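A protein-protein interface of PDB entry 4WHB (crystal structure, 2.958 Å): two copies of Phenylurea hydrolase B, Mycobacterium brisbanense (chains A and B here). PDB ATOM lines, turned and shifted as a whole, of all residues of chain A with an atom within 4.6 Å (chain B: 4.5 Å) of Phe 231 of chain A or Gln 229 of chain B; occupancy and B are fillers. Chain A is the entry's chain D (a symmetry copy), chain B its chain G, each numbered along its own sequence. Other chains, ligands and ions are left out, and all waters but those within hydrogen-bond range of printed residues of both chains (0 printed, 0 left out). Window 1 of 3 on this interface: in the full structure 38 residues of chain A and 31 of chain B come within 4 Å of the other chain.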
ATOM      1  N   VAL A 144      22.480   6.046  11.600  1.00  0.00           N
ATOM      2  CA  VAL A 144      22.935   5.168  12.656  1.00  0.00           C
ATOM      3  C   VAL A 144      21.733   4.848  13.553  1.00  0.00           C
ATOM      4  O   VAL A 144      20.973   5.758  13.955  1.00  0.00           O
ATOM      5  CB  VAL A 144      24.103   5.803  13.435  1.00  0.00           C
ATOM      6  CG1 VAL A 144      25.303   6.011  12.510  1.00  0.00           C
ATOM      7  CG2 VAL A 144      23.685   7.097  14.157  1.00  0.00           C
ATOM      8  N   GLY A 145      21.556   3.559  13.844  1.00  0.00           N
ATOM      9  CA  GLY A 145      20.379   3.116  14.605  1.00  0.00           C
ATOM     10  C   GLY A 145      19.330   2.407  13.759  1.00  0.00           C
ATOM     11  O   GLY A 145      18.400   1.768  14.314  1.00  0.00           O
ATOM     12  N   LEU A 182      24.054  -1.793  17.275  1.00  0.00           N
ATOM     13  CA  LEU A 182      23.956  -0.463  17.889  1.00  0.00           C
ATOM     14  C   LEU A 182      22.939  -0.426  19.042  1.00  0.00           C
ATOM     15  O   LEU A 182      23.101   0.338  19.999  1.00  0.00           O
ATOM     16  CB  LEU A 182      23.637   0.619  16.854  1.00  0.00           C
ATOM     17  CG  LEU A 182      24.735   1.240  15.981  1.00  0.00           C
ATOM     18  CD1 LEU A 182      25.003   2.703  16.387  1.00  0.00           C
ATOM     19  CD2 LEU A 182      26.040   0.427  15.927  1.00  0.00           C
ATOM     20  N   SER A 183      21.883  -1.237  18.933  1.00  0.00           N
ATOM     21  CA  SER A 183      20.836  -1.344  19.937  1.00  0.00           C
ATOM     22  C   SER A 183      21.327  -2.252  21.023  1.00  0.00           C
ATOM     23  O   SER A 183      21.155  -1.975  22.198  1.00  0.00           O
ATOM     24  CB  SER A 183      19.534  -1.898  19.319  1.00  0.00           C
ATOM     25  OG  SER A 183      18.535  -0.885  19.216  1.00  0.00           O
ATOM     26  N   ILE A 207      20.811  10.243  13.409  1.00  0.00           N
ATOM     27  CA  ILE A 207      20.711   9.148  14.363  1.00  0.00           C
ATOM     28  C   ILE A 207      19.212   8.929  14.489  1.00  0.00           C
ATOM     29  O   ILE A 207      18.435   9.894  14.616  1.00  0.00           O
ATOM     30  CB  ILE A 207      21.406   9.518  15.719  1.00  0.00           C
ATOM     31  CG1 ILE A 207      21.277   8.412  16.725  1.00  0.00           C
ATOM     32  CG2 ILE A 207      20.835  10.783  16.314  1.00  0.00           C
ATOM     33  CD1 ILE A 207      21.939   8.759  18.050  1.00  0.00           C
ATOM     34  N   ALA A 208      18.774   7.680  14.446  1.00  0.00           N
ATOM     35  CA  ALA A 208      17.351   7.462  14.543  1.00  0.00           C
ATOM     36  C   ALA A 208      16.952   7.423  15.989  1.00  0.00           C
ATOM     37  O   ALA A 208      17.192   6.408  16.655  1.00  0.00           O
ATOM     38  CB  ALA A 208      16.939   6.186  13.845  1.00  0.00           C
ATOM     39  N   TYR A 228       8.879   3.445  19.531  1.00  0.00           N
ATOM     40  CA  TYR A 228       9.956   3.138  20.479  1.00  0.00           C
ATOM     41  C   TYR A 228      11.112   4.088  20.236  1.00  0.00           C
ATOM     42  O   TYR A 228      11.199   4.681  19.163  1.00  0.00           O
ATOM     43  CB  TYR A 228      10.435   1.713  20.264  1.00  0.00           C
ATOM     44  CG  TYR A 228       9.438   0.634  20.565  1.00  0.00           C
ATOM     45  CD1 TYR A 228       8.095   0.925  20.848  1.00  0.00           C
ATOM     46  CD2 TYR A 228       9.820  -0.709  20.484  1.00  0.00           C
ATOM     47  CE1 TYR A 228       7.195  -0.100  21.096  1.00  0.00           C
ATOM     48  CE2 TYR A 228       8.933  -1.728  20.698  1.00  0.00           C
ATOM     49  CZ  TYR A 228       7.632  -1.431  20.986  1.00  0.00           C
ATOM     50  OH  TYR A 228       6.775  -2.472  21.211  1.00  0.00           O
ATOM     51  N   GLN A 229      11.993   4.230  21.226  1.00  0.00           N
ATOM     52  CA  GLN A 229      13.197   5.066  21.093  1.00  0.00           C
ATOM     53  C   GLN A 229      14.447   4.197  21.083  1.00  0.00           C
ATOM     54  O   GLN A 229      14.817   3.604  22.100  1.00  0.00           O
ATOM     55  CB  GLN A 229      13.260   6.096  22.198  1.00  0.00           C
ATOM     56  CG  GLN A 229      11.903   6.708  22.459  1.00  0.00           C
ATOM     57  CD  GLN A 229      11.978   8.114  22.940  1.00  0.00           C
ATOM     58  OE1 GLN A 229      10.903   8.891  22.672  1.00  0.00           O
ATOM     59  NE2 GLN A 229      12.989   8.513  23.558  1.00  0.00           N
ATOM     60  N   THR A 230      15.083   4.142  19.914  1.00  0.00           N
ATOM     61  CA  THR A 230      16.040   3.098  19.582  1.00  0.00           C
ATOM     62  C   THR A 230      17.180   2.837  20.601  1.00  0.00           C
ATOM     63  O   THR A 230      17.584   1.688  20.866  1.00  0.00           O
ATOM     64  CB  THR A 230      16.666   3.369  18.209  1.00  0.00           C
ATOM     65  OG1 THR A 230      15.737   4.036  17.378  1.00  0.00           O
ATOM     66  CG2 THR A 230      17.115   2.013  17.569  1.00  0.00           C
ATOM     67  N   PHE A 231      17.725   3.920  21.144  1.00  0.00           N
ATOM     68  CA  PHE A 231      18.794   3.812  22.123  1.00  0.00           C
ATOM     69  C   PHE A 231      18.445   4.523  23.397  1.00  0.00           C
ATOM     70  O   PHE A 231      17.530   5.363  23.442  1.00  0.00           O
ATOM     71  CB  PHE A 231      20.082   4.420  21.607  1.00  0.00           C
ATOM     72  CG  PHE A 231      20.479   3.964  20.256  1.00  0.00           C
ATOM     73  CD1 PHE A 231      20.000   4.610  19.136  1.00  0.00           C
ATOM     74  CD2 PHE A 231      21.378   2.949  20.109  1.00  0.00           C
ATOM     75  CE1 PHE A 231      20.396   4.226  17.858  1.00  0.00           C
ATOM     76  CE2 PHE A 231      21.782   2.565  18.865  1.00  0.00           C
ATOM     77  CZ  PHE A 231      21.287   3.187  17.734  1.00  0.00           C
ATOM     78  N   SER A 232      19.220   4.199  24.427  1.00  0.00           N
ATOM     79  CA  SER A 232      19.135   4.865  25.721  1.00  0.00           C
ATOM     80  C   SER A 232      19.764   6.216  25.600  1.00  0.00           C
ATOM     81  O   SER A 232      20.491   6.462  24.649  1.00  0.00           O
ATOM     82  CB  SER A 232      19.858   4.031  26.763  1.00  0.00           C
ATOM     83  OG  SER A 232      20.930   3.320  26.150  1.00  0.00           O
ATOM     84  N   ARG A 233      19.463   7.071  26.571  1.00  0.00           N
ATOM     85  CA  ARG A 233      20.006   8.421  26.619  1.00  0.00           C
ATOM     86  C   ARG A 233      21.556   8.454  26.689  1.00  0.00           C
ATOM     87  O   ARG A 233      22.162   9.311  26.045  1.00  0.00           O
ATOM     88  CB  ARG A 233      19.435   9.151  27.802  1.00  0.00           C
ATOM     89  CG  ARG A 233      19.766  10.631  27.824  1.00  0.00           C
ATOM     90  CD  ARG A 233      18.996  11.411  26.760  1.00  0.00           C
ATOM     91  NE  ARG A 233      18.642  12.743  27.266  1.00  0.00           N
ATOM     92  CZ  ARG A 233      19.536  13.704  27.559  1.00  0.00           C
ATOM     93  NH1 ARG A 233      20.815  13.485  27.376  1.00  0.00           N
ATOM     94  NH2 ARG A 233      19.162  14.868  28.087  1.00  0.00           N
ATOM     95  N   VAL A 235      23.654   6.573  25.305  1.00  0.00           N
ATOM     96  CA  VAL A 235      24.143   6.325  23.951  1.00  0.00           C
ATOM     97  C   VAL A 235      23.844   7.477  23.009  1.00  0.00           C
ATOM     98  O   VAL A 235      24.670   7.786  22.175  1.00  0.00           O
ATOM     99  CB  VAL A 235      23.507   5.055  23.363  1.00  0.00           C
ATOM    100  CG1 VAL A 235      24.016   4.810  21.979  1.00  0.00           C
ATOM    101  CG2 VAL A 235      23.774   3.859  24.257  1.00  0.00           C
ATOM    102  N   LEU A 236      22.660   8.083  23.100  1.00  0.00           N
ATOM    103  CA  LEU A 236      22.306   9.132  22.171  1.00  0.00           C
ATOM    104  C   LEU A 236      23.261  10.283  22.312  1.00  0.00           C
ATOM    105  O   LEU A 236      23.768  10.761  21.315  1.00  0.00           O
ATOM    106  CB  LEU A 236      20.885   9.583  22.355  1.00  0.00           C
ATOM    107  CG  LEU A 236      19.847   9.071  21.330  1.00  0.00           C
ATOM    108  CD1 LEU A 236      20.087   7.590  21.052  1.00  0.00           C
ATOM    109  CD2 LEU A 236      18.419   9.267  21.834  1.00  0.00           C
ATOM    110  N   MET A 239      26.916   9.510  21.230  1.00  0.00           N
ATOM    111  CA  MET A 239      27.158   9.731  19.826  1.00  0.00           C
ATOM    112  C   MET A 239      27.409  11.207  19.548  1.00  0.00           C
ATOM    113  O   MET A 239      28.416  11.562  18.963  1.00  0.00           O
ATOM    114  CB  MET A 239      25.974   9.256  19.001  1.00  0.00           C
ATOM    115  CG  MET A 239      25.369   7.909  19.399  1.00  0.00           C
ATOM    116  SD  MET A 239      24.896   6.877  18.009  1.00  0.00           S
ATOM    117  CE  MET A 239      23.754   5.751  18.793  1.00  0.00           C
ATOM    118  N   VAL B 209      10.895  -1.698  29.763  1.00  0.00           N
ATOM    119  CA  VAL B 209      11.835  -0.642  29.402  1.00  0.00           C
ATOM    120  C   VAL B 209      12.076  -0.731  27.926  1.00  0.00           C
ATOM    121  O   VAL B 209      12.212   0.277  27.233  1.00  0.00           O
ATOM    122  CB  VAL B 209      13.183  -0.818  30.161  1.00  0.00           C
ATOM    123  CG1 VAL B 209      14.240   0.183  29.693  1.00  0.00           C
ATOM    124  CG2 VAL B 209      12.966  -0.677  31.651  1.00  0.00           C
ATOM    125  N   SER B 210      12.129  -1.973  27.463  1.00  0.00           N
ATOM    126  CA  SER B 210      12.443  -2.293  26.091  1.00  0.00           C
ATOM    127  C   SER B 210      11.392  -3.217  25.487  1.00  0.00           C
ATOM    128  O   SER B 210      10.535  -3.737  26.208  1.00  0.00           O
ATOM    129  CB  SER B 210      13.835  -2.889  25.989  1.00  0.00           C
ATOM    130  OG  SER B 210      14.046  -3.886  26.938  1.00  0.00           O
ATOM    131  N   SER B 227      16.736  -4.516  19.461  1.00  0.00           N
ATOM    132  CA  SER B 227      16.084  -4.396  20.789  1.00  0.00           C
ATOM    133  C   SER B 227      15.038  -3.295  20.846  1.00  0.00           C
ATOM    134  O   SER B 227      13.849  -3.594  21.121  1.00  0.00           O
ATOM    135  CB  SER B 227      17.100  -4.220  21.921  1.00  0.00           C
ATOM    136  OG  SER B 227      16.534  -4.604  23.154  1.00  0.00           O
ATOM    137  N   TYR B 228      15.480  -2.058  20.586  1.00  0.00           N
ATOM    138  CA  TYR B 228      14.676  -0.828  20.873  1.00  0.00           C
ATOM    139  C   TYR B 228      14.365  -0.555  22.355  1.00  0.00           C
ATOM    140  O   TYR B 228      14.888  -1.182  23.280  1.00  0.00           O
ATOM    141  CB  TYR B 228      13.303  -0.816  20.163  1.00  0.00           C
ATOM    142  CG  TYR B 228      13.302  -0.607  18.682  1.00  0.00           C
ATOM    143  CD1 TYR B 228      13.697   0.601  18.145  1.00  0.00           C
ATOM    144  CD2 TYR B 228      12.884  -1.594  17.822  1.00  0.00           C
ATOM    145  CE1 TYR B 228      13.706   0.813  16.781  1.00  0.00           C
ATOM    146  CE2 TYR B 228      12.901  -1.400  16.454  1.00  0.00           C
ATOM    147  CZ  TYR B 228      13.303  -0.195  15.941  1.00  0.00           C
ATOM    148  OH  TYR B 228      13.311   0.061  14.603  1.00  0.00           O
ATOM    149  N   GLN B 229      13.522   0.448  22.536  1.00  0.00           N
ATOM    150  CA  GLN B 229      13.110   0.914  23.844  1.00  0.00           C
ATOM    151  C   GLN B 229      11.778   1.649  23.707  1.00  0.00           C
ATOM    152  O   GLN B 229      11.667   2.557  22.882  1.00  0.00           O
ATOM    153  CB  GLN B 229      14.174   1.846  24.483  1.00  0.00           C
ATOM    154  CG  GLN B 229      15.221   1.085  25.291  1.00  0.00           C
ATOM    155  CD  GLN B 229      16.308   1.964  25.866  1.00  0.00           C
ATOM    156  OE1 GLN B 229      17.475   1.627  25.761  1.00  0.00           O
ATOM    157  NE2 GLN B 229      15.938   3.089  26.501  1.00  0.00           N
ATOM    158  N   THR B 230      10.818   1.329  24.579  1.00  0.00           N
ATOM    159  CA  THR B 230       9.486   1.857  24.441  1.00  0.00           C
ATOM    160  C   THR B 230       9.281   3.299  25.010  1.00  0.00           C
ATOM    161  O   THR B 230       8.613   4.141  24.396  1.00  0.00           O
ATOM    162  CB  THR B 230       8.462   0.891  25.054  1.00  0.00           C
ATOM    163  OG1 THR B 230       8.116   1.309  26.355  1.00  0.00           O
ATOM    164  CG2 THR B 230       8.975  -0.482  25.134  1.00  0.00           C
ATOM    165  N   PHE B 231       9.829   3.579  26.184  1.00  0.00           N
ATOM    166  CA  PHE B 231       9.662   4.911  26.724  1.00  0.00           C
ATOM    167  C   PHE B 231      10.975   5.681  26.753  1.00  0.00           C
ATOM    168  O   PHE B 231      12.049   5.112  26.578  1.00  0.00           O
ATOM    169  CB  PHE B 231       9.065   4.914  28.124  1.00  0.00           C
ATOM    170  CG  PHE B 231       7.833   4.081  28.270  1.00  0.00           C
ATOM    171  CD1 PHE B 231       6.626   4.592  27.888  1.00  0.00           C
ATOM    172  CD2 PHE B 231       7.880   2.833  28.847  1.00  0.00           C
ATOM    173  CE1 PHE B 231       5.465   3.872  28.032  1.00  0.00           C
ATOM    174  CE2 PHE B 231       6.755   2.091  28.995  1.00  0.00           C
ATOM    175  CZ  PHE B 231       5.533   2.608  28.576  1.00  0.00           C
ATOM    176  N   GLU B 258      22.074  -2.597  26.713  1.00  0.00           N
ATOM    177  CA  GLU B 258      21.377  -1.362  27.008  1.00  0.00           C
ATOM    178  C   GLU B 258      20.027  -1.790  27.568  1.00  0.00           C
ATOM    179  O   GLU B 258      19.512  -2.834  27.201  1.00  0.00           O
ATOM    180  CB  GLU B 258      21.195  -0.524  25.724  1.00  0.00           C
ATOM    181  CG  GLU B 258      22.398   0.336  25.381  1.00  0.00           C
ATOM    182  CD  GLU B 258      22.990   0.987  26.630  1.00  0.00           C
ATOM    183  OE1 GLU B 258      22.557   2.072  27.031  1.00  0.00           O
ATOM    184  OE2 GLU B 258      23.907   0.422  27.251  1.00  0.00           O
ATOM    185  N   ALA B 259      19.465  -0.991  28.456  1.00  0.00           N
ATOM    186  CA  ALA B 259      18.158  -1.273  29.058  1.00  0.00           C
ATOM    187  C   ALA B 259      18.224  -2.164  30.302  1.00  0.00           C
ATOM    188  O   ALA B 259      17.199  -2.481  30.893  1.00  0.00           O
ATOM    189  CB  ALA B 259      17.179  -1.844  28.034  1.00  0.00           C
ATOM    190  N   THR B 262      19.978   0.820  32.159  1.00  0.00           N
ATOM    191  CA  THR B 262      18.833   1.692  32.201  1.00  0.00           C
ATOM    192  C   THR B 262      17.821   1.261  33.244  1.00  0.00           C
ATOM    193  O   THR B 262      17.228   2.096  33.920  1.00  0.00           O
ATOM    194  CB  THR B 262      18.129   1.728  30.849  1.00  0.00           C
ATOM    195  OG1 THR B 262      19.088   2.040  29.842  1.00  0.00           O
ATOM    196  CG2 THR B 262      17.063   2.776  30.830  1.00  0.00           C
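Of chain B, only Gln 229 (3.9 Å) comes within 4 Å of Phe 231 of chain A. Of chain A, only Tyr 228, Gln 229, Phe 231 and Ser 232 come within 4 Å of Gln 229 of chain B. Of the printed residues of chain B, Tyr 228 of chain A touches Tyr 228, Gln 229 and Thr 230. Of the printed residues of chain A, Tyr 228 of chain B touches Ser 183 (3.5 Å), Tyr 228 (3.5 Å) and Thr 230 (3.7 Å). Of the printed residues of chain B, Gln 229 of chain A touches Gln 229 (2.4 Å). Ile 207 of chain A touches none of the printed residues of chain B. The nearest printed residue of chain B that does not touch Phe 231 of chain A is Tyr 228 of chain B (5.6 Å). The nearest printed residue of chain A that does not touch Gln 229 of chain B is Thr 230 of chain A (4.6 Å). The nearest printed residue of chain A that does not touch Ser 227 of chain B is Tyr 228 of chain A (5.0 Å).
OE1 of Glu 258 of chain B lies close to OG of Ser 232 of chain A. The backbone NH of Ser 232 of chain A sits at hydrogen-bond distance from the side-chain amide oxygen of Gln 229 of chain B. The backbone NH (N) of Gln 229 of chain B lies close to the backbone carbonyl oxygen (O) of Gln 229 of chain A, at 3.4 Å.
OG1 of Thr 230 of chain A is in hydrogen-bond range of O of Ala 208 of chain A (2.9 Å). N of Ala 259 of chain B sits at hydrogen-bond distance from OG1 of Thr 262 of chain B, 3.4 Å away. The backbone carbonyl oxygen (O) of Val 209 of chain B lies within hydrogen-bond range of the backbone NH (N) of Thr 230 of chain B (3.2 Å). O of Thr 230 of chain A lies within hydrogen-bond range of OG of Ser 183 of chain A, 3.2 Å away.
Among the printed residues, merely in contact across the chains: Ser 183 of chain A with Ser 227 of chain B (3.8 Å), Ser 183 of chain A with Tyr 228 of chain B (3.5 Å), Ser 183 of chain A with Glu 258 of chain B (3.8 Å), Tyr 228 of chain A with Tyr 228 of chain B (3.5 Å), Tyr 228 of chain A with Gln 229 of chain B (3.0 Å), Tyr 228 of chain A with Thr 230 of chain B (3.96 Å), Thr 230 of chain A with Tyr 228 of chain B (3.7 Å), Phe 231 of chain A with Gln 229 of chain B (3.9 Å), Ser 232 of chain A with Thr 262 of chain B (3.7 Å) and Val 235 of chain A with Glu 258 of chain B (3.5 Å).
Hydrophobic or aromatic side chains of chain A within 4 Å of the printed part of chain B: Tyr 228 and Val 235.
Tyr 228 of chain B touches its own counterpart, Tyr 228 of chain A. Tyr 228 of chain A touches Thr 230 of chain B, and with the chains exchanged Thr 230 of chain A touches Tyr 228 of chain B. Gln 229 of chain A touches its own counterpart, Gln 229 of chain B. Phe 231 of chain A touches Gln 229 of chain B, but with the chains exchanged Gln 229 of chain A does not touch Phe 231 of chain B (4.4 Å). 4 positions are printed for both chains. Of the 13 pairs that touch across the chains among the printed residues, 4 have their exchanged pair printed and touching as well.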
